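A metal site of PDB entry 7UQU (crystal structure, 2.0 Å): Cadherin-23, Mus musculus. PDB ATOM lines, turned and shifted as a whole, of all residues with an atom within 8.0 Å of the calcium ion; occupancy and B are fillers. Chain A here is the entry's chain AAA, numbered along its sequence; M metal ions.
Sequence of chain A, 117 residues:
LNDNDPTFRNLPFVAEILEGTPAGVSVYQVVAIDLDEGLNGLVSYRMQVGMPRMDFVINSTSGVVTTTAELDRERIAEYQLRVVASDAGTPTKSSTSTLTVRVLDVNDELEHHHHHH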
ATOM      1  N   LEU A   1       7.934 -20.125  30.915  1.00  0.00           N
ATOM      2  CA  LEU A   1       6.939 -19.287  31.653  1.00  0.00           C
ATOM      3  C   LEU A   1       7.064 -17.820  31.222  1.00  0.00           C
ATOM      4  O   LEU A   1       7.644 -17.572  30.144  1.00  0.00           O
ATOM      5  CB  LEU A   1       7.165 -19.470  33.162  1.00  0.00           C
ATOM      6  CG  LEU A   1       6.444 -20.661  33.784  1.00  0.00           C
ATOM      7  CD1 LEU A   1       6.911 -20.891  35.214  1.00  0.00           C
ATOM      8  CD2 LEU A   1       4.923 -20.483  33.725  1.00  0.00           C
ATOM      9  N   ASN A   2       6.522 -16.894  32.015  1.00  0.00           N
ATOM     10  CA  ASN A   2       6.510 -15.437  31.713  1.00  0.00           C
ATOM     11  C   ASN A   2       7.818 -14.798  32.194  1.00  0.00           C
ATOM     12  O   ASN A   2       7.849 -14.298  33.334  1.00  0.00           O
ATOM     13  CB  ASN A   2       5.271 -14.778  32.341  1.00  0.00           C
ATOM     14  CG  ASN A   2       4.908 -13.478  31.658  1.00  0.00           C
ATOM     15  OD1 ASN A   2       5.610 -13.050  30.746  1.00  0.00           O
ATOM     16  ND2 ASN A   2       3.818 -12.852  32.072  1.00  0.00           N
ATOM     17  N   ASP A   3       8.854 -14.764  31.348  1.00  0.00           N
ATOM     18  CA  ASP A   3      10.202 -14.254  31.699  1.00  0.00           C
ATOM     19  C   ASP A   3      10.206 -12.717  31.749  1.00  0.00           C
ATOM     20  O   ASP A   3      10.628 -12.149  32.780  1.00  0.00           O
ATOM     21  CB  ASP A   3      11.264 -14.695  30.691  1.00  0.00           C
ATOM     22  CG  ASP A   3      11.275 -16.188  30.381  1.00  0.00           C
ATOM     23  OD1 ASP A   3      10.279 -16.871  30.721  1.00  0.00           O
ATOM     24  OD2 ASP A   3      12.287 -16.652  29.816  1.00  0.00           O
ATOM     25  N   ASN A   4       9.742 -12.083  30.674  1.00  0.00           N
ATOM     26  CA  ASN A   4      10.002 -10.657  30.342  1.00  0.00           C
ATOM     27  C   ASN A   4       8.759  -9.814  30.622  1.00  0.00           C
ATOM     28  O   ASN A   4       7.640 -10.256  30.265  1.00  0.00           O
ATOM     29  CB  ASN A   4      10.421 -10.509  28.873  1.00  0.00           C
ATOM     30  CG  ASN A   4      11.555 -11.442  28.508  1.00  0.00           C
ATOM     31  OD1 ASN A   4      12.646 -11.330  29.053  1.00  0.00           O
ATOM     32  ND2 ASN A   4      11.306 -12.358  27.587  1.00  0.00           N
ATOM     33  N   ASP A   5       8.941  -8.648  31.254  1.00  0.00           N
ATOM     34  CA  ASP A   5       7.924  -7.560  31.257  1.00  0.00           C
ATOM     35  C   ASP A   5       7.937  -6.934  29.878  1.00  0.00           C
ATOM     36  O   ASP A   5       8.981  -6.872  29.243  1.00  0.00           O
ATOM     37  CB  ASP A   5       8.187  -6.461  32.281  1.00  0.00           C
ATOM     38  CG  ASP A   5       8.677  -6.957  33.623  1.00  0.00           C
ATOM     39  OD1 ASP A   5       9.845  -7.408  33.681  1.00  0.00           O
ATOM     40  OD2 ASP A   5       7.885  -6.916  34.586  1.00  0.00           O
ATOM     41  N   PRO A   6       6.806  -6.392  29.394  1.00  0.00           N
ATOM     42  CA  PRO A   6       6.812  -5.619  28.164  1.00  0.00           C
ATOM     43  C   PRO A   6       7.817  -4.480  28.352  1.00  0.00           C
ATOM     44  O   PRO A   6       7.975  -3.998  29.462  1.00  0.00           O
ATOM     45  CB  PRO A   6       5.361  -5.133  28.019  1.00  0.00           C
ATOM     46  CG  PRO A   6       4.564  -6.092  28.857  1.00  0.00           C
ATOM     47  CD  PRO A   6       5.466  -6.470  30.007  1.00  0.00           C
ATOM     48  N   ILE A  33       6.865  -3.877  23.543  1.00  0.00           N
ATOM     49  CA  ILE A  33       7.192  -5.225  22.991  1.00  0.00           C
ATOM     50  C   ILE A  33       7.513  -6.138  24.179  1.00  0.00           C
ATOM     51  O   ILE A  33       8.034  -5.656  25.209  1.00  0.00           O
ATOM     52  CB  ILE A  33       8.353  -5.099  21.996  1.00  0.00           C
ATOM     53  CG1 ILE A  33       7.810  -4.552  20.674  1.00  0.00           C
ATOM     54  CG2 ILE A  33       9.081  -6.425  21.809  1.00  0.00           C
ATOM     55  CD1 ILE A  33       8.860  -3.995  19.808  1.00  0.00           C
ATOM     56  N   ASP A  34       7.147  -7.399  24.010  1.00  0.00           N
ATOM     57  CA  ASP A  34       7.372  -8.476  24.988  1.00  0.00           C
ATOM     58  C   ASP A  34       8.089  -9.598  24.232  1.00  0.00           C
ATOM     59  O   ASP A  34       7.573 -10.013  23.179  1.00  0.00           O
ATOM     60  CB  ASP A  34       6.035  -8.864  25.614  1.00  0.00           C
ATOM     61  CG  ASP A  34       6.218  -9.703  26.855  1.00  0.00           C
ATOM     62  OD1 ASP A  34       6.854 -10.761  26.735  1.00  0.00           O
ATOM     63  OD2 ASP A  34       5.740  -9.275  27.931  1.00  0.00           O
ATOM     64  N   LEU A  35       9.261 -10.019  24.706  1.00  0.00           N
ATOM     65  CA  LEU A  35      10.101 -11.084  24.080  1.00  0.00           C
ATOM     66  C   LEU A  35       9.429 -12.465  24.225  1.00  0.00           C
ATOM     67  O   LEU A  35       9.645 -13.302  23.336  1.00  0.00           O
ATOM     68  CB  LEU A  35      11.479 -11.072  24.739  1.00  0.00           C
ATOM     69  CG  LEU A  35      12.512 -10.157  24.085  1.00  0.00           C
ATOM     70  CD1 LEU A  35      13.572  -9.716  25.088  1.00  0.00           C
ATOM     71  CD2 LEU A  35      13.149 -10.837  22.876  1.00  0.00           C
ATOM     72  N   ASP A  36       8.641 -12.684  25.281  1.00  0.00           N
ATOM     73  CA  ASP A  36       8.036 -14.005  25.611  1.00  0.00           C
ATOM     74  C   ASP A  36       7.109 -14.474  24.484  1.00  0.00           C
ATOM     75  O   ASP A  36       6.768 -13.658  23.599  1.00  0.00           O
ATOM     76  CB  ASP A  36       7.285 -13.973  26.947  1.00  0.00           C
ATOM     77  CG  ASP A  36       8.169 -13.671  28.142  1.00  0.00           C
ATOM     78  OD1 ASP A  36       9.390 -13.924  28.058  1.00  0.00           O
ATOM     79  OD2 ASP A  36       7.634 -13.187  29.160  1.00  0.00           O
ATOM     80  N   GLU A  37       6.725 -15.756  24.540  1.00  0.00           N
ATOM     81  CA  GLU A  37       6.009 -16.489  23.460  1.00  0.00           C
ATOM     82  C   GLU A  37       4.499 -16.410  23.711  1.00  0.00           C
ATOM     83  O   GLU A  37       4.105 -16.421  24.898  1.00  0.00           O
ATOM     84  CB  GLU A  37       6.458 -17.957  23.423  1.00  0.00           C
ATOM     85  CG  GLU A  37       6.645 -18.501  22.015  1.00  0.00           C
ATOM     86  CD  GLU A  37       7.945 -18.078  21.349  1.00  0.00           C
ATOM     87  OE1 GLU A  37       8.991 -18.104  22.034  1.00  0.00           O
ATOM     88  OE2 GLU A  37       7.913 -17.722  20.161  1.00  0.00           O
ATOM     89  N   GLY A  38       3.708 -16.332  22.632  1.00  0.00           N
ATOM     90  CA  GLY A  38       2.244 -16.452  22.640  1.00  0.00           C
ATOM     91  C   GLY A  38       1.574 -15.529  23.647  1.00  0.00           C
ATOM     92  O   GLY A  38       1.763 -14.299  23.557  1.00  0.00           O
ATOM     93  N   LEU A  39       0.806 -16.111  24.570  1.00  0.00           N
ATOM     94  CA  LEU A  39      -0.042 -15.373  25.552  1.00  0.00           C
ATOM     95  C   LEU A  39       0.871 -14.549  26.468  1.00  0.00           C
ATOM     96  O   LEU A  39       0.489 -13.407  26.814  1.00  0.00           O
ATOM     97  CB  LEU A  39      -0.895 -16.381  26.339  1.00  0.00           C
ATOM     98  CG  LEU A  39      -2.309 -15.915  26.722  1.00  0.00           C
ATOM     99  CD1 LEU A  39      -3.166 -15.684  25.492  1.00  0.00           C
ATOM    100  CD2 LEU A  39      -2.973 -16.906  27.662  1.00  0.00           C
ATOM    101  N   ASN A  40       2.062 -15.078  26.793  1.00  0.00           N
ATOM    102  CA  ASN A  40       3.092 -14.414  27.653  1.00  0.00           C
ATOM    103  C   ASN A  40       3.656 -13.145  26.990  1.00  0.00           C
ATOM    104  O   ASN A  40       4.274 -12.344  27.719  1.00  0.00           O
ATOM    105  CB  ASN A  40       4.235 -15.348  28.011  1.00  0.00           C
ATOM    106  CG  ASN A  40       3.876 -16.359  29.084  1.00  0.00           C
ATOM    107  OD1 ASN A  40       2.887 -16.191  29.800  1.00  0.00           O
ATOM    108  ND2 ASN A  40       4.694 -17.392  29.211  1.00  0.00           N
ATOM    109  N   GLY A  41       3.491 -12.971  25.665  1.00  0.00           N
ATOM    110  CA  GLY A  41       3.989 -11.801  24.923  1.00  0.00           C
ATOM    111  C   GLY A  41       2.949 -11.141  24.030  1.00  0.00           C
ATOM    112  O   GLY A  41       3.329 -10.541  23.017  1.00  0.00           O
ATOM    113  N   LEU A  42       1.662 -11.255  24.365  1.00  0.00           N
ATOM    114  CA  LEU A  42       0.574 -10.458  23.729  1.00  0.00           C
ATOM    115  C   LEU A  42       0.400  -9.211  24.596  1.00  0.00           C
ATOM    116  O   LEU A  42       0.013  -9.376  25.747  1.00  0.00           O
ATOM    117  CB  LEU A  42      -0.712 -11.288  23.666  1.00  0.00           C
ATOM    118  CG  LEU A  42      -1.996 -10.546  23.280  1.00  0.00           C
ATOM    119  CD1 LEU A  42      -2.101 -10.361  21.771  1.00  0.00           C
ATOM    120  CD2 LEU A  42      -3.219 -11.283  23.805  1.00  0.00           C
ATOM    121  N   VAL A  43       0.667  -8.025  24.061  1.00  0.00           N
ATOM    122  CA  VAL A  43       0.656  -6.761  24.868  1.00  0.00           C
ATOM    123  C   VAL A  43      -0.711  -6.085  24.758  1.00  0.00           C
ATOM    124  O   VAL A  43      -1.260  -6.033  23.667  1.00  0.00           O
ATOM    125  CB  VAL A  43       1.775  -5.823  24.398  1.00  0.00           C
ATOM    126  CG1 VAL A  43       1.646  -4.415  25.000  1.00  0.00           C
ATOM    127  CG2 VAL A  43       3.144  -6.410  24.699  1.00  0.00           C
ATOM    128  N   SER A  86       0.698  -4.348  29.488  1.00  0.00           N
ATOM    129  CA  SER A  86       0.597  -5.647  30.200  1.00  0.00           C
ATOM    130  C   SER A  86       0.644  -6.781  29.168  1.00  0.00           C
ATOM    131  O   SER A  86       0.087  -6.581  28.065  1.00  0.00           O
ATOM    132  CB  SER A  86      -0.671  -5.759  31.011  1.00  0.00           C
ATOM    133  OG  SER A  86      -0.824  -4.667  31.891  1.00  0.00           O
ATOM    134  N   ASP A  87       1.279  -7.906  29.507  1.00  0.00           N
ATOM    135  CA  ASP A  87       1.181  -9.163  28.719  1.00  0.00           C
ATOM    136  C   ASP A  87      -0.052  -9.939  29.211  1.00  0.00           C
ATOM    137  O   ASP A  87      -0.644  -9.518  30.217  1.00  0.00           O
ATOM    138  CB  ASP A  87       2.492  -9.952  28.736  1.00  0.00           C
ATOM    139  CG  ASP A  87       2.974 -10.415  30.104  1.00  0.00           C
ATOM    140  OD1 ASP A  87       2.119 -10.619  30.988  1.00  0.00           O
ATOM    141  OD2 ASP A  87       4.210 -10.580  30.260  1.00  0.00           O
ATOM    142  N   ALA A  88      -0.430 -11.009  28.513  1.00  0.00           N
ATOM    143  CA  ALA A  88      -1.567 -11.880  28.907  1.00  0.00           C
ATOM    144  C   ALA A  88      -1.045 -13.135  29.633  1.00  0.00           C
ATOM    145  O   ALA A  88      -1.776 -14.136  29.668  1.00  0.00           O
ATOM    146  CB  ALA A  88      -2.405 -12.216  27.697  1.00  0.00           C
ATOM    147  N   GLY A  89       0.144 -13.063  30.233  1.00  0.00           N
ATOM    148  CA  GLY A  89       0.776 -14.154  31.000  1.00  0.00           C
ATOM    149  C   GLY A  89      -0.024 -14.522  32.233  1.00  0.00           C
ATOM    150  O   GLY A  89      -0.669 -13.621  32.802  1.00  0.00           O
ATOM    151  N   PRO A  91       0.702 -15.359  35.402  1.00  0.00           N
ATOM    152  CA  PRO A  91       1.010 -14.173  36.205  1.00  0.00           C
ATOM    153  C   PRO A  91       1.221 -13.013  35.218  1.00  0.00           C
ATOM    154  O   PRO A  91       2.051 -13.144  34.326  1.00  0.00           O
ATOM    155  CB  PRO A  91       2.265 -14.615  36.979  1.00  0.00           C
ATOM    156  CG  PRO A  91       2.982 -15.540  35.996  1.00  0.00           C
ATOM    157  CD  PRO A  91       1.901 -16.164  35.128  1.00  0.00           C
ATOM    158  N   THR A  92       0.431 -11.958  35.338  1.00  0.00           N
ATOM    159  CA  THR A  92       0.460 -10.775  34.436  1.00  0.00           C
ATOM    160  C   THR A  92       1.698  -9.917  34.740  1.00  0.00           C
ATOM    161  O   THR A  92       1.862  -9.511  35.907  1.00  0.00           O
ATOM    162  CB  THR A  92      -0.852  -9.982  34.559  1.00  0.00           C
ATOM    163  OG1 THR A  92      -0.825  -8.992  33.529  1.00  0.00           O
ATOM    164  CG2 THR A  92      -1.034  -9.297  35.898  1.00  0.00           C
ATOM    165  N   LYS A  93       2.558  -9.664  33.731  1.00  0.00           N
ATOM    166  CA  LYS A  93       3.721  -8.733  33.819  1.00  0.00           C
ATOM    167  C   LYS A  93       3.388  -7.423  33.081  1.00  0.00           C
ATOM    168  O   LYS A  93       2.740  -7.453  32.014  1.00  0.00           O
ATOM    169  CB  LYS A  93       4.998  -9.376  33.279  1.00  0.00           C
ATOM    170  CG  LYS A  93       5.553 -10.499  34.146  1.00  0.00           C
ATOM    171  CD  LYS A  93       6.826 -11.104  33.622  1.00  0.00           C
ATOM    172  CE  LYS A  93       7.796 -11.492  34.718  1.00  0.00           C
ATOM    173  NZ  LYS A  93       8.502 -10.294  35.262  1.00  0.00           N
ATOM    174  N   SER A  94       3.802  -6.290  33.649  1.00  0.00           N
ATOM    175  CA  SER A  94       3.413  -4.953  33.148  1.00  0.00           C
ATOM    176  C   SER A  94       4.528  -3.935  33.413  1.00  0.00           C
ATOM    177  O   SER A  94       5.399  -4.207  34.273  1.00  0.00           O
ATOM    178  CB  SER A  94       2.094  -4.555  33.720  1.00  0.00           C
ATOM    179  OG  SER A  94       2.221  -4.177  35.081  1.00  0.00           O
HETATM  180 CA    CA M   1       5.937 -11.482  29.083  1.00  0.00          CA
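The backbone NH of Asp 87 lies within hydrogen-bond range of the backbone carbonyl oxygen of Lys 93 (2.9 Å).
The backbone NH (N) of Gly 89 is in hydrogen-bond range of the side-chain carboxylate (OD1) of Asp 87.
O of Asp 87 sits at hydrogen-bond distance from OG1 of Thr 92 (3.4 Å).
ND2 of Asn 2 is in hydrogen-bond range of O of Pro 91 (2.9 Å).
The backbone carbonyl oxygen (O) of Leu 1 sits at hydrogen-bond distance from the side-chain amide nitrogen (ND2) of Asn 40 (3.1 Å).
The backbone NH (N) of Asp 3 lies close to the side-chain carboxylate (OD1) of Asp 36 (3.4 Å).
Within 4 Å of the calcium ion: Asn 2, Asn 4, Asp 34, Asp 36, Asn 40 and Asp 87.
The calcium ion is bound by the side-chain carboxylate (OD2) of Asp 87 (2.3 Å).
The calcium ion is bound by the side-chain amide oxygen (OD1) of Asn 2, at 2.3 Å.
The calcium ion is bound by O of Asn 40 (2.3 Å).
OD2 of Asp 36 binds the calcium ion (2.4 Å).
The backbone carbonyl oxygen (O) of Asn 4 binds the calcium ion.
The side-chain carboxylate (OD2) of Asp 34 binds the calcium ion.
The calcium ion is bound by the side-chain carboxylate (OD1) of Asp 34.
The calcium ion has seven donor atoms within binding distance.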
